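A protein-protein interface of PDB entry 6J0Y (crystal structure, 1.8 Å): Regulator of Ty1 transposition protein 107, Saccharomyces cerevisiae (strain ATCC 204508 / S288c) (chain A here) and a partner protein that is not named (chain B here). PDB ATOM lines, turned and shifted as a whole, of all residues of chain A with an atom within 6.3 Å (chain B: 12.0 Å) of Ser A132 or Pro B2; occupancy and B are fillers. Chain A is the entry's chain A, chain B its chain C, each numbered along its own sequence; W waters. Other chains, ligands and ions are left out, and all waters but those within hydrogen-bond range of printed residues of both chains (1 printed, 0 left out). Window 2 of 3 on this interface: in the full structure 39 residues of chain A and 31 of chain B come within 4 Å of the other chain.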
ATOM      1  N   ILE A 129      -6.157 -22.221  13.298  1.00  0.00           N
ATOM      2  CA  ILE A 129      -6.317 -23.334  12.354  1.00  0.00           C
ATOM      3  C   ILE A 129      -7.327 -22.918  11.279  1.00  0.00           C
ATOM      4  O   ILE A 129      -8.469 -22.562  11.593  1.00  0.00           O
ATOM      5  CB  ILE A 129      -6.753 -24.617  13.079  1.00  0.00           C
ATOM      6  CG1 ILE A 129      -5.731 -24.960  14.185  1.00  0.00           C
ATOM      7  CG2 ILE A 129      -6.906 -25.786  12.074  1.00  0.00           C
ATOM      8  CD1 ILE A 129      -6.089 -26.182  15.008  1.00  0.00           C
ATOM      9  N   SER A 130      -6.912 -22.954  10.007  1.00  0.00           N
ATOM     10  CA  SER A 130      -7.744 -22.418   8.922  1.00  0.00           C
ATOM     11  C   SER A 130      -8.918 -23.333   8.607  1.00  0.00           C
ATOM     12  O   SER A 130      -8.737 -24.488   8.199  1.00  0.00           O
ATOM     13  CB  SER A 130      -6.930 -22.198   7.652  1.00  0.00           C
ATOM     14  OG  SER A 130      -7.805 -21.825   6.572  1.00  0.00           O
ATOM     15  N   LYS A 131     -10.132 -22.784   8.707  1.00  0.00           N
ATOM     16  CA  LYS A 131     -11.313 -23.561   8.373  1.00  0.00           C
ATOM     17  C   LYS A 131     -11.549 -23.654   6.873  1.00  0.00           C
ATOM     18  O   LYS A 131     -12.421 -24.421   6.450  1.00  0.00           O
ATOM     19  CB  LYS A 131     -12.536 -22.969   9.075  1.00  0.00           C
ATOM     20  CG  LYS A 131     -12.534 -23.268  10.565  1.00  0.00           C
ATOM     21  CD  LYS A 131     -13.601 -22.483  11.314  1.00  0.00           C
ATOM     22  CE  LYS A 131     -13.614 -22.886  12.788  1.00  0.00           C
ATOM     23  NZ  LYS A 131     -14.328 -21.904  13.663  1.00  0.00           N
ATOM     24  N   SER A 132     -10.790 -22.920   6.060  1.00  0.00           N
ATOM     25  CA  SER A 132     -10.852 -23.121   4.622  1.00  0.00           C
ATOM     26  C   SER A 132      -9.822 -24.138   4.141  1.00  0.00           C
ATOM     27  O   SER A 132      -9.791 -24.450   2.946  1.00  0.00           O
ATOM     28  CB  SER A 132     -10.705 -21.782   3.868  1.00  0.00           C
ATOM     29  OG  SER A 132      -9.665 -20.970   4.378  1.00  0.00           O
ATOM     30  N   SER A 133      -9.005 -24.687   5.048  1.00  0.00           N
ATOM     31  CA  SER A 133      -8.138 -25.817   4.719  1.00  0.00           C
ATOM     32  C   SER A 133      -8.709 -27.165   5.137  1.00  0.00           C
ATOM     33  O   SER A 133      -8.388 -28.180   4.509  1.00  0.00           O
ATOM     34  CB  SER A 133      -6.761 -25.665   5.402  1.00  0.00           C
ATOM     35  OG  SER A 133      -5.812 -25.030   4.561  1.00  0.00           O
ATOM     36  N   PHE A 134      -9.485 -27.225   6.212  1.00  0.00           N
ATOM     37  CA  PHE A 134      -9.778 -28.493   6.869  1.00  0.00           C
ATOM     38  C   PHE A 134     -11.273 -28.688   7.049  1.00  0.00           C
ATOM     39  O   PHE A 134     -12.001 -27.736   7.344  1.00  0.00           O
ATOM     40  CB  PHE A 134      -9.082 -28.563   8.243  1.00  0.00           C
ATOM     41  CG  PHE A 134      -7.614 -28.266   8.173  1.00  0.00           C
ATOM     42  CD1 PHE A 134      -6.762 -29.129   7.507  1.00  0.00           C
ATOM     43  CD2 PHE A 134      -7.091 -27.118   8.751  1.00  0.00           C
ATOM     44  CE1 PHE A 134      -5.409 -28.859   7.412  1.00  0.00           C
ATOM     45  CE2 PHE A 134      -5.740 -26.838   8.658  1.00  0.00           C
ATOM     46  CZ  PHE A 134      -4.895 -27.701   7.997  1.00  0.00           C
ATOM     47  N   ASN A 135     -11.716 -29.941   6.926  1.00  0.00           N
ATOM     48  CA  ASN A 135     -13.092 -30.266   7.280  1.00  0.00           C
ATOM     49  C   ASN A 135     -13.235 -30.343   8.800  1.00  0.00           C
ATOM     50  O   ASN A 135     -12.267 -30.176   9.551  1.00  0.00           O
ATOM     51  CB  ASN A 135     -13.549 -31.547   6.574  1.00  0.00           C
ATOM     52  CG  ASN A 135     -12.757 -32.784   6.980  1.00  0.00           C
ATOM     53  OD1 ASN A 135     -12.363 -32.955   8.134  1.00  0.00           O
ATOM     54  ND2 ASN A 135     -12.552 -33.675   6.020  1.00  0.00           N
ATOM     55  N   LYS A 136     -14.464 -30.591   9.270  1.00  0.00           N
ATOM     56  CA  LYS A 136     -14.727 -30.478  10.703  1.00  0.00           C
ATOM     57  C   LYS A 136     -13.972 -31.534  11.507  1.00  0.00           C
ATOM     58  O   LYS A 136     -13.491 -31.245  12.612  1.00  0.00           O
ATOM     59  CB  LYS A 136     -16.230 -30.575  10.990  1.00  0.00           C
ATOM     60  CG  LYS A 136     -16.622 -30.036  12.377  1.00  0.00           C
ATOM     61  CD  LYS A 136     -18.048 -30.436  12.788  1.00  0.00           C
ATOM     62  CE  LYS A 136     -18.401 -29.953  14.204  1.00  0.00           C
ATOM     63  NZ  LYS A 136     -19.739 -30.445  14.669  1.00  0.00           N
ATOM     64  N   GLU A 138     -11.085 -33.018  10.753  1.00  0.00           N
ATOM     65  CA  GLU A 138      -9.667 -32.648  10.786  1.00  0.00           C
ATOM     66  C   GLU A 138      -9.424 -31.503  11.764  1.00  0.00           C
ATOM     67  O   GLU A 138      -8.469 -31.525  12.556  1.00  0.00           O
ATOM     68  CB  GLU A 138      -9.205 -32.245   9.385  1.00  0.00           C
ATOM     69  CG  GLU A 138      -9.154 -33.401   8.388  1.00  0.00           C
ATOM     70  CD  GLU A 138      -8.887 -32.951   6.957  1.00  0.00           C
ATOM     71  OE1 GLU A 138      -8.219 -33.701   6.226  1.00  0.00           O
ATOM     72  OE2 GLU A 138      -9.353 -31.862   6.548  1.00  0.00           O
ATOM     73  N   ASP A 171      -5.035 -22.709  -0.120  1.00  0.00           N
ATOM     74  CA  ASP A 171      -5.954 -22.079   0.837  1.00  0.00           C
ATOM     75  C   ASP A 171      -5.995 -20.568   0.618  1.00  0.00           C
ATOM     76  O   ASP A 171      -4.955 -19.907   0.732  1.00  0.00           O
ATOM     77  CB  ASP A 171      -5.515 -22.397   2.276  1.00  0.00           C
ATOM     78  CG  ASP A 171      -6.572 -22.018   3.323  1.00  0.00           C
ATOM     79  OD1 ASP A 171      -7.421 -21.142   3.050  1.00  0.00           O
ATOM     80  OD2 ASP A 171      -6.545 -22.587   4.438  1.00  0.00           O
ATOM     81  N   PRO A 172      -7.161 -19.972   0.338  1.00  0.00           N
ATOM     82  CA  PRO A 172      -7.210 -18.509   0.145  1.00  0.00           C
ATOM     83  C   PRO A 172      -6.883 -17.701   1.397  1.00  0.00           C
ATOM     84  O   PRO A 172      -6.635 -16.491   1.282  1.00  0.00           O
ATOM     85  CB  PRO A 172      -8.657 -18.261  -0.314  1.00  0.00           C
ATOM     86  CG  PRO A 172      -9.426 -19.414   0.249  1.00  0.00           C
ATOM     87  CD  PRO A 172      -8.489 -20.599   0.245  1.00  0.00           C
ATOM     88  N   ILE A 173      -6.846 -18.319   2.580  1.00  0.00           N
ATOM     89  CA  ILE A 173      -6.489 -17.570   3.782  1.00  0.00           C
ATOM     90  C   ILE A 173      -5.057 -17.056   3.717  1.00  0.00           C
ATOM     91  O   ILE A 173      -4.720 -16.075   4.388  1.00  0.00           O
ATOM     92  CB  ILE A 173      -6.697 -18.425   5.047  1.00  0.00           C
ATOM     93  CG1 ILE A 173      -6.931 -17.503   6.247  1.00  0.00           C
ATOM     94  CG2 ILE A 173      -5.471 -19.364   5.308  1.00  0.00           C
ATOM     95  CD1 ILE A 173      -7.118 -18.219   7.574  1.00  0.00           C
ATOM     96  N   GLY B   1     -17.083 -29.629   3.435  1.00  0.00           N
ATOM     97  CA  GLY B   1     -16.181 -29.515   4.568  1.00  0.00           C
ATOM     98  C   GLY B   1     -15.655 -28.114   4.816  1.00  0.00           C
ATOM     99  O   GLY B   1     -16.210 -27.376   5.631  1.00  0.00           O
ATOM    100  N   PRO B   2     -14.581 -27.744   4.119  1.00  0.00           N
ATOM    101  CA  PRO B   2     -13.927 -26.458   4.399  1.00  0.00           C
ATOM    102  C   PRO B   2     -14.724 -25.274   3.874  1.00  0.00           C
ATOM    103  O   PRO B   2     -15.348 -25.339   2.813  1.00  0.00           O
ATOM    104  CB  PRO B   2     -12.579 -26.578   3.669  1.00  0.00           C
ATOM    105  CG  PRO B   2     -12.429 -28.042   3.326  1.00  0.00           C
ATOM    106  CD  PRO B   2     -13.825 -28.546   3.142  1.00  0.00           C
ATOM    107  N   LEU B   3     -14.689 -24.181   4.636  1.00  0.00           N
ATOM    108  CA  LEU B   3     -15.267 -22.917   4.195  1.00  0.00           C
ATOM    109  C   LEU B   3     -14.650 -22.481   2.869  1.00  0.00           C
ATOM    110  O   LEU B   3     -13.484 -22.764   2.578  1.00  0.00           O
ATOM    111  CB  LEU B   3     -15.044 -21.842   5.259  1.00  0.00           C
ATOM    112  CG  LEU B   3     -15.879 -21.939   6.540  1.00  0.00           C
ATOM    113  CD1 LEU B   3     -15.335 -21.011   7.627  1.00  0.00           C
ATOM    114  CD2 LEU B   3     -17.339 -21.606   6.241  1.00  0.00           C
ATOM    115  N   GLY B   4     -15.443 -21.785   2.055  1.00  0.00           N
ATOM    116  CA  GLY B   4     -15.031 -21.456   0.702  1.00  0.00           C
ATOM    117  C   GLY B   4     -15.264 -19.994   0.368  1.00  0.00           C
ATOM    118  O   GLY B   4     -15.103 -19.102   1.201  1.00  0.00           O
ATOM    119  N   SER B   5     -15.656 -19.763  -0.885  1.00  0.00           N
ATOM    120  CA  SER B   5     -15.793 -18.413  -1.419  1.00  0.00           C
ATOM    121  C   SER B   5     -16.851 -17.624  -0.654  1.00  0.00           C
ATOM    122  O   SER B   5     -17.887 -18.161  -0.253  1.00  0.00           O
ATOM    123  CB  SER B   5     -16.153 -18.485  -2.909  1.00  0.00           C
ATOM    124  OG  SER B   5     -16.030 -17.229  -3.552  1.00  0.00           O
ATOM    125  N   GLY B   6     -16.582 -16.335  -0.449  1.00  0.00           N
ATOM    126  CA  GLY B   6     -17.512 -15.464   0.236  1.00  0.00           C
ATOM    127  C   GLY B   6     -17.468 -15.531   1.745  1.00  0.00           C
ATOM    128  O   GLY B   6     -18.057 -14.661   2.407  1.00  0.00           O
ATOM    129  N   SER B   7     -16.807 -16.535   2.323  1.00  0.00           N
ATOM    130  CA  SER B   7     -16.685 -16.575   3.773  1.00  0.00           C
ATOM    131  C   SER B   7     -15.649 -15.555   4.235  1.00  0.00           C
ATOM    132  O   SER B   7     -14.959 -14.918   3.432  1.00  0.00           O
ATOM    133  CB  SER B   7     -16.310 -17.979   4.251  1.00  0.00           C
ATOM    134  OG  SER B   7     -15.020 -18.333   3.795  1.00  0.00           O
ATOM    135  N   SER B   8     -15.536 -15.412   5.556  1.00  0.00           N
ATOM    136  CA  SER B   8     -14.686 -14.399   6.151  1.00  0.00           C
ATOM    137  C   SER B   8     -13.871 -14.995   7.290  1.00  0.00           C
ATOM    138  O   SER B   8     -14.106 -16.117   7.744  1.00  0.00           O
ATOM    139  CB  SER B   8     -15.510 -13.215   6.680  1.00  0.00           C
ATOM    140  OG  SER B   8     -16.374 -13.628   7.723  1.00  0.00           O
ATOM    141  N   ILE B   9     -12.911 -14.201   7.753  1.00  0.00           N
ATOM    142  CA  ILE B   9     -12.126 -14.534   8.935  1.00  0.00           C
ATOM    143  C   ILE B   9     -12.212 -13.355   9.886  1.00  0.00           C
ATOM    144  O   ILE B   9     -12.421 -12.210   9.469  1.00  0.00           O
ATOM    145  CB  ILE B   9     -10.654 -14.846   8.596  1.00  0.00           C
ATOM    146  CG1 ILE B   9      -9.998 -13.629   7.929  1.00  0.00           C
ATOM    147  CG2 ILE B   9     -10.550 -16.094   7.700  1.00  0.00           C
ATOM    148  CD1 ILE B   9      -8.505 -13.827   7.657  1.00  0.00           C
ATOM    149  N   ARG B  10     -12.013 -13.641  11.169  1.00  0.00           N
ATOM    150  CA  ARG B  10     -12.007 -12.635  12.230  1.00  0.00           C
ATOM    151  C   ARG B  10     -10.602 -12.072  12.399  1.00  0.00           C
ATOM    152  O   ARG B  10      -9.646 -12.838  12.510  1.00  0.00           O
ATOM    153  CB  ARG B  10     -12.460 -13.265  13.550  1.00  0.00           C
ATOM    154  CG  ARG B  10     -13.972 -13.532  13.623  1.00  0.00           C
ATOM    155  CD  ARG B  10     -14.289 -14.731  14.522  1.00  0.00           C
ATOM    156  NE  ARG B  10     -13.597 -14.753  15.817  1.00  0.00           N
ATOM    157  CZ  ARG B  10     -13.804 -13.904  16.821  1.00  0.00           C
ATOM    158  NH1 ARG B  10     -14.664 -12.890  16.695  1.00  0.00           N
ATOM    159  NH2 ARG B  10     -13.118 -14.076  17.953  1.00  0.00           N
ATOM    160  N   ILE B  54     -13.232 -10.143   7.662  1.00  0.00           N
ATOM    161  CA  ILE B  54     -12.568  -9.831   6.406  1.00  0.00           C
ATOM    162  C   ILE B  54     -12.878 -10.961   5.433  1.00  0.00           C
ATOM    163  O   ILE B  54     -12.605 -12.132   5.725  1.00  0.00           O
ATOM    164  CB  ILE B  54     -11.053  -9.659   6.605  1.00  0.00           C
ATOM    165  CG1 ILE B  54     -10.760  -8.543   7.624  1.00  0.00           C
ATOM    166  CG2 ILE B  54     -10.360  -9.415   5.262  1.00  0.00           C
ATOM    167  CD1 ILE B  54     -11.106  -7.149   7.138  1.00  0.00           C
ATOM    168  N   GLN B  55     -13.460 -10.625   4.282  1.00  0.00           N
ATOM    169  CA  GLN B  55     -13.737 -11.644   3.276  1.00  0.00           C
ATOM    170  C   GLN B  55     -12.451 -12.271   2.739  1.00  0.00           C
ATOM    171  O   GLN B  55     -11.469 -11.574   2.456  1.00  0.00           O
ATOM    172  CB  GLN B  55     -14.536 -11.025   2.124  1.00  0.00           C
ATOM    173  CG  GLN B  55     -14.960 -11.985   1.051  1.00  0.00           C
ATOM    174  CD  GLN B  55     -15.865 -11.302   0.049  1.00  0.00           C
ATOM    175  OE1 GLN B  55     -17.038 -11.063   0.325  1.00  0.00           O
ATOM    176  NE2 GLN B  55     -15.315 -10.944  -1.100  1.00  0.00           N
ATOM    177  N   LEU B  56     -12.468 -13.598   2.563  1.00  0.00           N
ATOM    178  CA  LEU B  56     -11.359 -14.278   1.899  1.00  0.00           C
ATOM    179  C   LEU B  56     -11.156 -13.720   0.495  1.00  0.00           C
ATOM    180  O   LEU B  56     -12.118 -13.495  -0.244  1.00  0.00           O
ATOM    181  CB  LEU B  56     -11.616 -15.786   1.812  1.00  0.00           C
ATOM    182  CG  LEU B  56     -11.663 -16.646   3.077  1.00  0.00           C
ATOM    183  CD1 LEU B  56     -11.908 -18.112   2.698  1.00  0.00           C
ATOM    184  CD2 LEU B  56     -10.366 -16.518   3.869  1.00  0.00           C
ATOM    185  N   VAL B  57      -9.895 -13.488   0.123  1.00  0.00           N
ATOM    186  CA  VAL B  57      -9.618 -12.923  -1.194  1.00  0.00           C
ATOM    187  C   VAL B  57      -9.934 -13.962  -2.261  1.00  0.00           C
ATOM    188  O   VAL B  57      -9.744 -15.169  -2.057  1.00  0.00           O
ATOM    189  CB  VAL B  57      -8.163 -12.430  -1.295  1.00  0.00           C
ATOM    190  CG1 VAL B  57      -7.842 -11.469  -0.152  1.00  0.00           C
ATOM    191  CG2 VAL B  57      -7.201 -13.591  -1.299  1.00  0.00           C
ATOM    192  N   ASP B  58     -10.451 -13.501  -3.396  1.00  0.00           N
ATOM    193  CA  ASP B  58     -10.935 -14.399  -4.444  1.00  0.00           C
ATOM    194  C   ASP B  58      -9.784 -15.092  -5.167  1.00  0.00           C
ATOM    195  O   ASP B  58      -8.945 -14.439  -5.788  1.00  0.00           O
ATOM    196  CB  ASP B  58     -11.802 -13.633  -5.449  1.00  0.00           C
ATOM    197  CG  ASP B  58     -13.024 -12.993  -4.802  1.00  0.00           C
ATOM    198  OD1 ASP B  58     -13.664 -13.642  -3.947  1.00  0.00           O
ATOM    199  OD2 ASP B  58     -13.345 -11.836  -5.150  1.00  0.00           O
HETATM  200  O   HOH W   1     -11.611 -23.487   0.664  1.00  0.00           O
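The backbone NH of Leu B3 sits at hydrogen-bond distance from the backbone carbonyl oxygen of Lys A131.
Of the printed residues of chain B, Ser A132 touches Pro B2 and Leu B3.
Pro B2 touches three residues of chain A.
No residue of chain B comes within 4 Å of Ser A133.
Of chain B, only Leu B56 and Val B57 come within 4 Å of Pro A172.
Of the printed residues of chain A, Leu B56 touches Pro A172 (3.7 Å).
Of the printed residues of chain A, Gly B1 touches Asn A135.
Of the printed residues of chain B, Lys A131 touches Pro B2 and Leu B3.
Of the printed residues of chain A, Leu B3 touches Lys A131 and Ser A132.
Printed residues of chain A within 4 Å of Val B57: Pro A172.
Ile B54 touches none of the printed residues of chain A.
The nearest printed residue of chain B that does not touch Ser A132 is Leu B56 (4.003 Å).
The nearest printed residue of chain A that does not touch Leu B3 is Phe A134 (5.2 Å).
Printed residues of chain A that touch a printed residue of chain B: Lys A131, Ser A132, Phe A134, Asn A135 and Pro A172.
Hydrophobic or aromatic side chains of chain B within 4 Å of the printed part of chain A: Pro B2, Leu B3, Leu B56 and Val B57.
Among the printed residues, 8 pairs touch across the chains.
Lys A131 touches Pro B2.
Ser A132 touches Pro B2.
Leu B3 touches Ser A132 (O to CB, 3.2 Å).
Pro B2 touches Phe A134 (CA to O, 3.7 Å).
CB of Asn A135 touches CA of Gly B1, at 3.9 Å.
CD1 of Leu B56 touches CG of Pro A172, 3.7 Å away.
CB of Pro A172 touches O of Val B57 (3.7 Å).
The side-chain hydroxyl (OG) of Ser A130 is in hydrogen-bond range of the side-chain hydroxyl (OG) of Ser A132 (3.0 Å).
OD1 of Asp A171 sits at hydrogen-bond distance from OG of Ser A132 (2.6 Å).
The side-chain amide oxygen (OD1) of Asn A135 sits at hydrogen-bond distance from the backbone NH (N) of Glu A138, 2.9 Å away.
The backbone carbonyl oxygen of Ser B7 is in hydrogen-bond range of the backbone NH of Leu B56 (3.0 Å).
Water W1 lies within hydrogen-bond range of the backbone carbonyl oxygen of Leu B3 and the backbone carbonyl oxygen of Ser A132.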
